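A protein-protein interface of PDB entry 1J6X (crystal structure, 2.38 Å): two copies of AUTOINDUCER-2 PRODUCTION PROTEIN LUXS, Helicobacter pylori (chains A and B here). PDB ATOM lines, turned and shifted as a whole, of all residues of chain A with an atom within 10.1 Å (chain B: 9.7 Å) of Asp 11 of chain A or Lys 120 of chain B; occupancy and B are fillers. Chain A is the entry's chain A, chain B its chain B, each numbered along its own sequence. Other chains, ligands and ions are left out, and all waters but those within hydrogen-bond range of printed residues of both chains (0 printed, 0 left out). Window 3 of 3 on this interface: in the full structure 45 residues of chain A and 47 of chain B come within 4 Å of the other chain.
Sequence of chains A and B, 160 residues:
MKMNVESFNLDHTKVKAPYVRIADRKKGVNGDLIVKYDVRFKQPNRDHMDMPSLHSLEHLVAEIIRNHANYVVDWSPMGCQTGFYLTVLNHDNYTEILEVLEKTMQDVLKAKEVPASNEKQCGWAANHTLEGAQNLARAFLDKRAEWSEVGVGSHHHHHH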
ATOM      1  N   MET A   1     -15.047  -5.466  38.536  1.00  0.00           N
ATOM      2  CA  MET A   1     -14.641  -6.774  37.944  1.00  0.00           C
ATOM      3  C   MET A   1     -14.227  -6.614  36.482  1.00  0.00           C
ATOM      4  O   MET A   1     -14.955  -6.019  35.691  1.00  0.00           O
ATOM      5  CB  MET A   1     -15.791  -7.781  38.032  1.00  0.00           C
ATOM      6  CG  MET A   1     -15.483  -9.092  37.322  1.00  0.00           C
ATOM      7  SD  MET A   1     -16.989 -10.297  37.070  1.00  0.00           S
ATOM      8  CE  MET A   1     -16.370 -11.788  38.161  1.00  0.00           C
ATOM      9  N   VAL A   5     -14.107  -9.249  27.776  1.00  0.00           N
ATOM     10  CA  VAL A   5     -14.247  -8.251  26.718  1.00  0.00           C
ATOM     11  C   VAL A   5     -13.745  -6.871  27.159  1.00  0.00           C
ATOM     12  O   VAL A   5     -14.216  -6.334  28.160  1.00  0.00           O
ATOM     13  CB  VAL A   5     -15.721  -8.148  26.307  1.00  0.00           C
ATOM     14  CG1 VAL A   5     -15.887  -7.122  25.210  1.00  0.00           C
ATOM     15  CG2 VAL A   5     -16.220  -9.510  25.869  1.00  0.00           C
ATOM     16  N   GLU A   6     -12.812  -6.286  26.406  1.00  0.00           N
ATOM     17  CA  GLU A   6     -12.250  -4.988  26.788  1.00  0.00           C
ATOM     18  C   GLU A   6     -13.207  -3.791  26.836  1.00  0.00           C
ATOM     19  O   GLU A   6     -13.043  -2.917  27.689  1.00  0.00           O
ATOM     20  CB  GLU A   6     -11.040  -4.638  25.906  1.00  0.00           C
ATOM     21  CG  GLU A   6     -11.338  -3.891  24.606  1.00  0.00           C
ATOM     22  CD  GLU A   6     -11.748  -2.424  24.809  1.00  0.00           C
ATOM     23  OE1 GLU A   6     -11.165  -1.725  25.680  1.00  0.00           O
ATOM     24  OE2 GLU A   6     -12.650  -1.968  24.072  1.00  0.00           O
ATOM     25  N   SER A   7     -14.190  -3.721  25.939  1.00  0.00           N
ATOM     26  CA  SER A   7     -15.089  -2.570  25.980  1.00  0.00           C
ATOM     27  C   SER A   7     -15.962  -2.583  27.227  1.00  0.00           C
ATOM     28  O   SER A   7     -16.489  -1.543  27.616  1.00  0.00           O
ATOM     29  CB  SER A   7     -15.956  -2.467  24.711  1.00  0.00           C
ATOM     30  OG  SER A   7     -16.770  -3.604  24.507  1.00  0.00           O
ATOM     31  N   PHE A   8     -16.105  -3.748  27.861  1.00  0.00           N
ATOM     32  CA  PHE A   8     -16.897  -3.844  29.091  1.00  0.00           C
ATOM     33  C   PHE A   8     -16.128  -3.174  30.230  1.00  0.00           C
ATOM     34  O   PHE A   8     -16.701  -2.873  31.285  1.00  0.00           O
ATOM     35  CB  PHE A   8     -17.159  -5.305  29.498  1.00  0.00           C
ATOM     36  CG  PHE A   8     -18.060  -6.067  28.559  1.00  0.00           C
ATOM     37  CD1 PHE A   8     -18.837  -5.406  27.606  1.00  0.00           C
ATOM     38  CD2 PHE A   8     -18.146  -7.453  28.652  1.00  0.00           C
ATOM     39  CE1 PHE A   8     -19.686  -6.112  26.760  1.00  0.00           C
ATOM     40  CE2 PHE A   8     -18.998  -8.177  27.809  1.00  0.00           C
ATOM     41  CZ  PHE A   8     -19.769  -7.502  26.859  1.00  0.00           C
ATOM     42  N   ASN A   9     -14.834  -2.947  30.011  1.00  0.00           N
ATOM     43  CA  ASN A   9     -13.968  -2.339  31.016  1.00  0.00           C
ATOM     44  C   ASN A   9     -13.837  -0.826  30.837  1.00  0.00           C
ATOM     45  O   ASN A   9     -13.119  -0.159  31.585  1.00  0.00           O
ATOM     46  CB  ASN A   9     -12.588  -3.020  30.989  1.00  0.00           C
ATOM     47  CG  ASN A   9     -12.677  -4.542  31.216  1.00  0.00           C
ATOM     48  OD1 ASN A   9     -11.933  -5.314  30.607  1.00  0.00           O
ATOM     49  ND2 ASN A   9     -13.583  -4.969  32.096  1.00  0.00           N
ATOM     50  N   LEU A  10     -14.539  -0.294  29.838  1.00  0.00           N
ATOM     51  CA  LEU A  10     -14.548   1.141  29.558  1.00  0.00           C
ATOM     52  C   LEU A  10     -15.741   1.738  30.286  1.00  0.00           C
ATOM     53  O   LEU A  10     -16.844   1.209  30.188  1.00  0.00           O
ATOM     54  CB  LEU A  10     -14.722   1.395  28.060  1.00  0.00           C
ATOM     55  CG  LEU A  10     -15.113   2.818  27.659  1.00  0.00           C
ATOM     56  CD1 LEU A  10     -13.940   3.762  27.902  1.00  0.00           C
ATOM     57  CD2 LEU A  10     -15.533   2.827  26.197  1.00  0.00           C
ATOM     58  N   ASP A  11     -15.526   2.835  31.005  1.00  0.00           N
ATOM     59  CA  ASP A  11     -16.612   3.480  31.738  1.00  0.00           C
ATOM     60  C   ASP A  11     -17.403   4.371  30.785  1.00  0.00           C
ATOM     61  O   ASP A  11     -17.057   5.526  30.572  1.00  0.00           O
ATOM     62  CB  ASP A  11     -16.050   4.316  32.901  1.00  0.00           C
ATOM     63  CG  ASP A  11     -17.121   4.729  33.900  1.00  0.00           C
ATOM     64  OD1 ASP A  11     -18.192   5.200  33.458  1.00  0.00           O
ATOM     65  OD2 ASP A  11     -16.891   4.593  35.123  1.00  0.00           O
ATOM     66  N   HIS A  12     -18.474   3.817  30.223  1.00  0.00           N
ATOM     67  CA  HIS A  12     -19.316   4.527  29.266  1.00  0.00           C
ATOM     68  C   HIS A  12     -19.957   5.808  29.770  1.00  0.00           C
ATOM     69  O   HIS A  12     -20.398   6.637  28.966  1.00  0.00           O
ATOM     70  CB  HIS A  12     -20.418   3.599  28.733  1.00  0.00           C
ATOM     71  CG  HIS A  12     -19.932   2.583  27.749  1.00  0.00           C
ATOM     72  ND1 HIS A  12     -19.188   1.484  28.117  1.00  0.00           N
ATOM     73  CD2 HIS A  12     -20.097   2.492  26.408  1.00  0.00           C
ATOM     74  CE1 HIS A  12     -18.917   0.758  27.049  1.00  0.00           C
ATOM     75  NE2 HIS A  12     -19.456   1.347  25.997  1.00  0.00           N
ATOM     76  N   THR A  13     -20.027   5.976  31.088  1.00  0.00           N
ATOM     77  CA  THR A  13     -20.628   7.186  31.641  1.00  0.00           C
ATOM     78  C   THR A  13     -19.636   8.343  31.729  1.00  0.00           C
ATOM     79  O   THR A  13     -20.000   9.440  32.143  1.00  0.00           O
ATOM     80  CB  THR A  13     -21.220   6.950  33.054  1.00  0.00           C
ATOM     81  OG1 THR A  13     -20.210   6.412  33.920  1.00  0.00           O
ATOM     82  CG2 THR A  13     -22.412   6.005  32.987  1.00  0.00           C
ATOM     83  N   LYS A  14     -18.389   8.106  31.331  1.00  0.00           N
ATOM     84  CA  LYS A  14     -17.371   9.155  31.393  1.00  0.00           C
ATOM     85  C   LYS A  14     -16.765   9.553  30.046  1.00  0.00           C
ATOM     86  O   LYS A  14     -15.844  10.374  29.980  1.00  0.00           O
ATOM     87  CB  LYS A  14     -16.268   8.735  32.368  1.00  0.00           C
ATOM     88  CG  LYS A  14     -16.760   8.682  33.815  1.00  0.00           C
ATOM     89  CD  LYS A  14     -15.688   8.197  34.771  1.00  0.00           C
ATOM     90  CE  LYS A  14     -16.244   8.060  36.174  1.00  0.00           C
ATOM     91  NZ  LYS A  14     -15.260   7.389  37.065  1.00  0.00           N
ATOM     92  N   VAL A  15     -17.282   8.975  28.970  1.00  0.00           N
ATOM     93  CA  VAL A  15     -16.777   9.302  27.651  1.00  0.00           C
ATOM     94  C   VAL A  15     -17.741  10.267  26.969  1.00  0.00           C
ATOM     95  O   VAL A  15     -18.911  10.361  27.347  1.00  0.00           O
ATOM     96  CB  VAL A  15     -16.596   8.031  26.800  1.00  0.00           C
ATOM     97  CG1 VAL A  15     -15.680   7.052  27.533  1.00  0.00           C
ATOM     98  CG2 VAL A  15     -17.945   7.392  26.510  1.00  0.00           C
ATOM     99  N   LYS A  16     -17.245  11.003  25.981  1.00  0.00           N
ATOM    100  CA  LYS A  16     -18.085  11.942  25.269  1.00  0.00           C
ATOM    101  C   LYS A  16     -17.995  11.776  23.760  1.00  0.00           C
ATOM    102  O   LYS A  16     -16.995  12.153  23.144  1.00  0.00           O
ATOM    103  CB  LYS A  16     -17.706  13.371  25.638  1.00  0.00           C
ATOM    104  CG  LYS A  16     -18.542  14.409  24.908  1.00  0.00           C
ATOM    105  CD  LYS A  16     -18.294  15.807  25.448  1.00  0.00           C
ATOM    106  CE  LYS A  16     -19.333  16.805  24.929  1.00  0.00           C
ATOM    107  NZ  LYS A  16     -19.277  18.078  25.714  1.00  0.00           N
ATOM    108  N   ALA A  17     -19.038  11.209  23.169  1.00  0.00           N
ATOM    109  CA  ALA A  17     -19.098  11.015  21.726  1.00  0.00           C
ATOM    110  C   ALA A  17     -19.208  12.393  21.084  1.00  0.00           C
ATOM    111  O   ALA A  17     -19.718  13.327  21.704  1.00  0.00           O
ATOM    112  CB  ALA A  17     -20.313  10.181  21.369  1.00  0.00           C
ATOM    113  N   TYR A  19     -15.973  10.302  19.046  1.00  0.00           N
ATOM    114  CA  TYR A  19     -14.552  10.170  19.339  1.00  0.00           C
ATOM    115  C   TYR A  19     -13.977   8.885  18.739  1.00  0.00           C
ATOM    116  O   TYR A  19     -14.729   7.953  18.434  1.00  0.00           O
ATOM    117  CB  TYR A  19     -14.333  10.188  20.869  1.00  0.00           C
ATOM    118  CG  TYR A  19     -14.809   8.935  21.590  1.00  0.00           C
ATOM    119  CD1 TYR A  19     -14.216   7.688  21.329  1.00  0.00           C
ATOM    120  CD2 TYR A  19     -15.876   8.977  22.497  1.00  0.00           C
ATOM    121  CE1 TYR A  19     -14.677   6.518  21.944  1.00  0.00           C
ATOM    122  CE2 TYR A  19     -16.342   7.802  23.121  1.00  0.00           C
ATOM    123  CZ  TYR A  19     -15.739   6.580  22.834  1.00  0.00           C
ATOM    124  OH  TYR A  19     -16.207   5.405  23.400  1.00  0.00           O
ATOM    125  N   ARG A  21     -11.184   6.081  19.732  1.00  0.00           N
ATOM    126  CA  ARG A  21     -10.374   5.630  20.852  1.00  0.00           C
ATOM    127  C   ARG A  21      -9.576   4.344  20.606  1.00  0.00           C
ATOM    128  O   ARG A  21     -10.087   3.389  20.028  1.00  0.00           O
ATOM    129  CB  ARG A  21     -11.304   5.462  22.066  1.00  0.00           C
ATOM    130  CG  ARG A  21     -10.699   4.792  23.299  1.00  0.00           C
ATOM    131  CD  ARG A  21     -11.776   4.541  24.382  1.00  0.00           C
ATOM    132  NE  ARG A  21     -12.633   3.406  24.043  1.00  0.00           N
ATOM    133  CZ  ARG A  21     -12.349   2.138  24.331  1.00  0.00           C
ATOM    134  NH1 ARG A  21     -11.230   1.831  24.980  1.00  0.00           N
ATOM    135  NH2 ARG A  21     -13.169   1.171  23.950  1.00  0.00           N
ATOM    136  N   ASP A  38     -12.081   2.112  18.815  1.00  0.00           N
ATOM    137  CA  ASP A  38     -13.475   2.354  19.165  1.00  0.00           C
ATOM    138  C   ASP A  38     -13.855   3.703  18.530  1.00  0.00           C
ATOM    139  O   ASP A  38     -13.459   4.752  19.036  1.00  0.00           O
ATOM    140  CB  ASP A  38     -13.597   2.415  20.703  1.00  0.00           C
ATOM    141  CG  ASP A  38     -14.934   2.978  21.190  1.00  0.00           C
ATOM    142  OD1 ASP A  38     -15.750   3.432  20.357  1.00  0.00           O
ATOM    143  OD2 ASP A  38     -15.160   2.978  22.428  1.00  0.00           O
ATOM    144  N   ARG A  40     -16.711   5.925  18.082  1.00  0.00           N
ATOM    145  CA  ARG A  40     -18.019   6.251  18.661  1.00  0.00           C
ATOM    146  C   ARG A  40     -18.719   7.434  17.997  1.00  0.00           C
ATOM    147  O   ARG A  40     -18.221   8.556  18.028  1.00  0.00           O
ATOM    148  CB  ARG A  40     -17.808   6.544  20.160  1.00  0.00           C
ATOM    149  CG  ARG A  40     -19.023   6.452  21.046  1.00  0.00           C
ATOM    150  CD  ARG A  40     -19.544   5.031  21.172  1.00  0.00           C
ATOM    151  NE  ARG A  40     -18.611   4.113  21.827  1.00  0.00           N
ATOM    152  CZ  ARG A  40     -18.994   2.999  22.451  1.00  0.00           C
ATOM    153  NH1 ARG A  40     -20.277   2.675  22.504  1.00  0.00           N
ATOM    154  NH2 ARG A  40     -18.107   2.203  23.017  1.00  0.00           N
ATOM    155  N   GLN A  43     -23.518   9.303  21.737  1.00  0.00           N
ATOM    156  CA  GLN A  43     -23.346   9.316  23.186  1.00  0.00           C
ATOM    157  C   GLN A  43     -24.034   8.084  23.792  1.00  0.00           C
ATOM    158  O   GLN A  43     -25.245   7.878  23.635  1.00  0.00           O
ATOM    159  CB  GLN A  43     -23.950  10.598  23.766  1.00  0.00           C
ATOM    160  CG  GLN A  43     -23.605  10.829  25.219  1.00  0.00           C
ATOM    161  CD  GLN A  43     -22.110  10.842  25.455  1.00  0.00           C
ATOM    162  OE1 GLN A  43     -21.378  11.648  24.872  1.00  0.00           O
ATOM    163  NE2 GLN A  43     -21.646   9.946  26.312  1.00  0.00           N
ATOM    164  N   PRO A  44     -23.259   7.233  24.482  1.00  0.00           N
ATOM    165  CA  PRO A  44     -23.792   6.019  25.105  1.00  0.00           C
ATOM    166  C   PRO A  44     -25.020   6.223  25.994  1.00  0.00           C
ATOM    167  O   PRO A  44     -25.038   7.080  26.876  1.00  0.00           O
ATOM    168  CB  PRO A  44     -22.597   5.488  25.878  1.00  0.00           C
ATOM    169  CG  PRO A  44     -21.459   5.884  25.003  1.00  0.00           C
ATOM    170  CD  PRO A  44     -21.798   7.303  24.648  1.00  0.00           C
ATOM    171  N   ASN A  45     -26.044   5.412  25.745  1.00  0.00           N
ATOM    172  CA  ASN A  45     -27.279   5.456  26.507  1.00  0.00           C
ATOM    173  C   ASN A  45     -27.984   6.797  26.492  1.00  0.00           C
ATOM    174  O   ASN A  45     -28.809   7.070  27.360  1.00  0.00           O
ATOM    175  CB  ASN A  45     -26.998   5.027  27.937  1.00  0.00           C
ATOM    176  CG  ASN A  45     -26.584   3.588  28.019  1.00  0.00           C
ATOM    177  OD1 ASN A  45     -27.390   2.698  27.781  1.00  0.00           O
ATOM    178  ND2 ASN A  45     -25.318   3.344  28.340  1.00  0.00           N
ATOM    179  N   VAL A 150     -11.640  11.783  24.110  1.00  0.00           N
ATOM    180  CA  VAL A 150     -12.566  10.734  24.527  1.00  0.00           C
ATOM    181  C   VAL A 150     -13.256  10.991  25.869  1.00  0.00           C
ATOM    182  O   VAL A 150     -14.427  10.643  26.045  1.00  0.00           O
ATOM    183  CB  VAL A 150     -11.841   9.367  24.620  1.00  0.00           C
ATOM    184  CG1 VAL A 150     -12.839   8.267  24.911  1.00  0.00           C
ATOM    185  CG2 VAL A 150     -11.086   9.085  23.329  1.00  0.00           C
ATOM    186  N   GLY A 151     -12.524  11.577  26.814  1.00  0.00           N
ATOM    187  CA  GLY A 151     -13.082  11.862  28.128  1.00  0.00           C
ATOM    188  C   GLY A 151     -13.906  13.139  28.172  1.00  0.00           C
ATOM    189  O   GLY A 151     -14.528  13.428  29.223  1.00  0.00           O
ATOM    190  N   HIS B  59     -22.884  -9.901  23.532  1.00  0.00           N
ATOM    191  CA  HIS B  59     -22.239  -9.785  24.841  1.00  0.00           C
ATOM    192  C   HIS B  59     -21.910 -11.167  25.373  1.00  0.00           C
ATOM    193  O   HIS B  59     -20.780 -11.420  25.781  1.00  0.00           O
ATOM    194  CB  HIS B  59     -23.146  -9.102  25.868  1.00  0.00           C
ATOM    195  CG  HIS B  59     -23.167  -7.608  25.783  1.00  0.00           C
ATOM    196  ND1 HIS B  59     -23.296  -6.807  26.898  1.00  0.00           N
ATOM    197  CD2 HIS B  59     -23.155  -6.773  24.719  1.00  0.00           C
ATOM    198  CE1 HIS B  59     -23.369  -5.542  26.524  1.00  0.00           C
ATOM    199  NE2 HIS B  59     -23.288  -5.495  25.206  1.00  0.00           N
ATOM    200  N   PRO B 115     -24.075 -10.426  30.459  1.00  0.00           N
ATOM    201  CA  PRO B 115     -22.864  -9.740  30.923  1.00  0.00           C
ATOM    202  C   PRO B 115     -22.765  -8.268  30.561  1.00  0.00           C
ATOM    203  O   PRO B 115     -23.094  -7.852  29.445  1.00  0.00           O
ATOM    204  CB  PRO B 115     -21.739 -10.528  30.271  1.00  0.00           C
ATOM    205  CG  PRO B 115     -22.325 -11.876  30.073  1.00  0.00           C
ATOM    206  CD  PRO B 115     -23.714 -11.568  29.608  1.00  0.00           C
ATOM    207  N   ALA B 116     -22.281  -7.498  31.525  1.00  0.00           N
ATOM    208  CA  ALA B 116     -22.080  -6.076  31.366  1.00  0.00           C
ATOM    209  C   ALA B 116     -23.248  -5.393  30.679  1.00  0.00           C
ATOM    210  O   ALA B 116     -23.049  -4.603  29.767  1.00  0.00           O
ATOM    211  CB  ALA B 116     -20.806  -5.849  30.574  1.00  0.00           C
ATOM    212  N   SER B 117     -24.464  -5.687  31.120  1.00  0.00           N
ATOM    213  CA  SER B 117     -25.640  -5.067  30.527  1.00  0.00           C
ATOM    214  C   SER B 117     -26.178  -3.916  31.402  1.00  0.00           C
ATOM    215  O   SER B 117     -27.309  -3.974  31.913  1.00  0.00           O
ATOM    216  CB  SER B 117     -26.746  -6.097  30.345  1.00  0.00           C
ATOM    217  OG  SER B 117     -27.081  -6.737  31.559  1.00  0.00           O
ATOM    218  N   ASN B 118     -25.377  -2.866  31.542  1.00  0.00           N
ATOM    219  CA  ASN B 118     -25.721  -1.698  32.332  1.00  0.00           C
ATOM    220  C   ASN B 118     -25.099  -0.513  31.588  1.00  0.00           C
ATOM    221  O   ASN B 118     -24.379  -0.693  30.622  1.00  0.00           O
ATOM    222  CB  ASN B 118     -25.103  -1.850  33.710  1.00  0.00           C
ATOM    223  CG  ASN B 118     -23.599  -1.922  33.632  1.00  0.00           C
ATOM    224  OD1 ASN B 118     -22.969  -0.980  33.139  1.00  0.00           O
ATOM    225  ND2 ASN B 118     -23.012  -3.031  34.062  1.00  0.00           N
ATOM    226  N   GLU B 119     -25.392   0.693  32.042  1.00  0.00           N
ATOM    227  CA  GLU B 119     -24.901   1.904  31.400  1.00  0.00           C
ATOM    228  C   GLU B 119     -23.406   2.186  31.541  1.00  0.00           C
ATOM    229  O   GLU B 119     -22.862   3.048  30.847  1.00  0.00           O
ATOM    230  CB  GLU B 119     -25.718   3.096  31.905  1.00  0.00           C
ATOM    231  CG  GLU B 119     -27.217   2.756  32.014  1.00  0.00           C
ATOM    232  CD  GLU B 119     -28.155   3.977  31.996  1.00  0.00           C
ATOM    233  OE1 GLU B 119     -27.831   5.057  32.560  1.00  0.00           O
ATOM    234  OE2 GLU B 119     -29.249   3.834  31.403  1.00  0.00           O
ATOM    235  N   LYS B 120     -22.738   1.475  32.440  1.00  0.00           N
ATOM    236  CA  LYS B 120     -21.307   1.681  32.627  1.00  0.00           C
ATOM    237  C   LYS B 120     -20.517   0.902  31.594  1.00  0.00           C
ATOM    238  O   LYS B 120     -19.485   1.368  31.131  1.00  0.00           O
ATOM    239  CB  LYS B 120     -20.842   1.219  34.016  1.00  0.00           C
ATOM    240  CG  LYS B 120     -20.920   2.265  35.104  1.00  0.00           C
ATOM    241  CD  LYS B 120     -20.196   1.801  36.365  1.00  0.00           C
ATOM    242  CE  LYS B 120     -20.322   2.836  37.498  1.00  0.00           C
ATOM    243  NZ  LYS B 120     -21.740   3.114  37.906  1.00  0.00           N
ATOM    244  N   GLN B 121     -21.012  -0.274  31.228  1.00  0.00           N
ATOM    245  CA  GLN B 121     -20.295  -1.128  30.289  1.00  0.00           C
ATOM    246  C   GLN B 121     -21.018  -1.402  28.973  1.00  0.00           C
ATOM    247  O   GLN B 121     -20.752  -2.411  28.320  1.00  0.00           O
ATOM    248  CB  GLN B 121     -19.984  -2.469  30.970  1.00  0.00           C
ATOM    249  CG  GLN B 121     -19.876  -2.405  32.484  1.00  0.00           C
ATOM    250  CD  GLN B 121     -19.599  -3.762  33.109  1.00  0.00           C
ATOM    251  OE1 GLN B 121     -18.459  -4.222  33.130  1.00  0.00           O
ATOM    252  NE2 GLN B 121     -20.648  -4.417  33.614  1.00  0.00           N
ATOM    253  N   CYS B 122     -21.907  -0.506  28.566  1.00  0.00           N
ATOM    254  CA  CYS B 122     -22.675  -0.731  27.349  1.00  0.00           C
ATOM    255  C   CYS B 122     -23.267   0.580  26.835  1.00  0.00           C
ATOM    256  O   CYS B 122     -23.648   1.437  27.627  1.00  0.00           O
ATOM    257  CB  CYS B 122     -23.772  -1.759  27.659  1.00  0.00           C
ATOM    258  SG  CYS B 122     -24.935  -2.066  26.353  1.00  0.00           S
ATOM    259  N   GLY B 123     -23.346   0.730  25.513  1.00  0.00           N
ATOM    260  CA  GLY B 123     -23.854   1.958  24.920  1.00  0.00           C
ATOM    261  C   GLY B 123     -25.357   2.071  24.801  1.00  0.00           C
ATOM    262  O   GLY B 123     -25.888   3.134  24.448  1.00  0.00           O
ATOM    263  N   TRP B 124     -26.038   0.960  25.061  1.00  0.00           N
ATOM    264  CA  TRP B 124     -27.497   0.896  25.025  1.00  0.00           C
ATOM    265  C   TRP B 124     -27.911  -0.265  25.930  1.00  0.00           C
ATOM    266  O   TRP B 124     -28.465  -1.270  25.472  1.00  0.00           O
ATOM    267  CB  TRP B 124     -28.011   0.648  23.605  1.00  0.00           C
ATOM    268  CG  TRP B 124     -29.450   1.064  23.454  1.00  0.00           C
ATOM    269  CD1 TRP B 124     -30.273   1.528  24.447  1.00  0.00           C
ATOM    270  CD2 TRP B 124     -30.236   1.060  22.253  1.00  0.00           C
ATOM    271  NE1 TRP B 124     -31.519   1.811  23.934  1.00  0.00           N
ATOM    272  CE2 TRP B 124     -31.524   1.532  22.593  1.00  0.00           C
ATOM    273  CE3 TRP B 124     -29.978   0.704  20.923  1.00  0.00           C
ATOM    274  CZ2 TRP B 124     -32.550   1.655  21.653  1.00  0.00           C
ATOM    275  CZ3 TRP B 124     -31.003   0.827  19.983  1.00  0.00           C
ATOM    276  CH2 TRP B 124     -32.273   1.298  20.356  1.00  0.00           C
ATOM    277  N   ALA B 125     -27.619  -0.107  27.218  1.00  0.00           N
ATOM    278  CA  ALA B 125     -27.888  -1.111  28.244  1.00  0.00           C
ATOM    279  C   ALA B 125     -29.325  -1.593  28.293  1.00  0.00           C
ATOM    280  O   ALA B 125     -29.594  -2.734  28.671  1.00  0.00           O
ATOM    281  CB  ALA B 125     -27.489  -0.566  29.619  1.00  0.00           C
ATOM    282  N   ALA B 126     -30.251  -0.720  27.919  1.00  0.00           N
ATOM    283  CA  ALA B 126     -31.661  -1.071  27.955  1.00  0.00           C
ATOM    284  C   ALA B 126     -32.022  -2.103  26.899  1.00  0.00           C
ATOM    285  O   ALA B 126     -32.753  -3.045  27.191  1.00  0.00           O
ATOM    286  CB  ALA B 126     -32.521   0.194  27.790  1.00  0.00           C
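Of the 23 printed residues of chain A, 7 touch a printed residue of chain B. Hydrophobic or aromatic side chains of chain A that line the printed part of chain B: Phe 8, His 12 and Pro 44. Of the 13 printed residues of chain B, 9 touch a printed residue of chain A. Among the printed residues, 17 pairs touch across the chains. Among the printed residues, no Asp or Glu carboxylate lies within 4 Å of a Lys or Arg side-chain nitrogen of the other chain.
No position is printed for both chains.
Phe 8 of chain A touches His 59 of chain B. CG of Phe 8 of chain A touches CB of Ala 116 of chain B (3.4 Å). Asp 11 of chain A touches Lys 120 of chain B (CA to O, 3.6 Å). Glu 119 of chain B touches His 12 of chain A (O to CB, 3.3 Å). His 12 of chain A touches Gln 121 of chain B (ND1 to C, 3.5 Å). His 12 of chain A touches Gly 123 of chain B. CG2 of Thr 13 of chain A touches O of Glu 119 of chain B, 3.7 Å away. Gly 123 of chain B touches Pro 44 of chain A. CA of Glu 119 of chain B touches ND2 of Asn 45 of chain A, at 3.4 Å.
The side-chain amide nitrogen (ND2) of Asn 118 of chain B sits close to the side-chain amide nitrogen (NE2) of Gln 121 of chain B (2.8 Å). O of Leu 10 of chain A sits at hydrogen-bond distance from ND1 of His 12 of chain A (3.1 Å). The side-chain carboxylate of Asp 11 of chain A sits close to the backbone NH of Thr 13 of chain A (3.1 Å). The side-chain sulfur of Cys 122 of chain B sits close to the backbone NH of Ala 125 of chain B. The side-chain carboxylate of Asp 11 of chain A lies within salt-bridge range of the side-chain amino group of Lys 14 of chain A (3.8 Å). The side-chain amide oxygen (OD1) of Asn 118 of chain B sits at hydrogen-bond distance from the backbone NH (N) of Lys 120 of chain B (2.6 Å).
OD1 of Asn 45 of chain A lies within hydrogen-bond range of N of Ala 125 of chain B (2.9 Å). The side-chain amide nitrogen (ND2) of Asn 45 of chain A is in hydrogen-bond range of the backbone carbonyl oxygen (O) of Cys 122 of chain B (2.6 Å). The backbone carbonyl oxygen (O) of Leu 10 of chain A sits close to the backbone carbonyl oxygen (O) of Lys 120 of chain B. O of Gly 123 of chain B sits at hydrogen-bond distance from N of Asn 45 of chain A. The backbone carbonyl oxygen (O) of Phe 8 of chain A lies close to the side-chain amide oxygen (OE1) of Gln 121 of chain B (2.9 Å). The backbone NH (N) of His 12 of chain A sits at hydrogen-bond distance from the backbone carbonyl oxygen (O) of Lys 120 of chain B. N of Cys 122 of chain B lies within hydrogen-bond range of ND1 of His 12 of chain A, 3.4 Å away. The backbone NH of Trp 124 of chain B sits close to the side-chain amide oxygen of Asn 45 of chain A, 3.5 Å away.
Of chain B, only Lys 120 (3.6 Å) comes within 4 Å of Asp 11 of chain A. Lys 120 of chain B touches just these residues of chain A: Leu 10 (2.8 Å), Asp 11 (3.6 Å) and His 12 (2.8 Å). Printed residues of chain B within 4 Å of His 12 of chain A: Glu 119, Lys 120, Gln 121, Cys 122 and Gly 123. Of chain B, only Glu 119 comes within 4 Å of Thr 13 of chain A. Of the printed residues of chain B, Phe 8 of chain A touches His 59, Ala 116 and Gln 121. Printed residues of chain A within 4 Å of His 59 of chain B: Phe 8 (3.6 Å). Of the printed residues of chain A, Cys 122 of chain B touches His 12 and Asn 45. Val 5 of chain A touches none of the printed residues of chain B. The nearest residue of chain A that does not touch Lys 120 of chain B is Thr 13 of chain A (4.4 Å). The nearest printed residue of chain B that does not touch Pro 44 of chain A is Cys 122 of chain B (4.5 Å).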
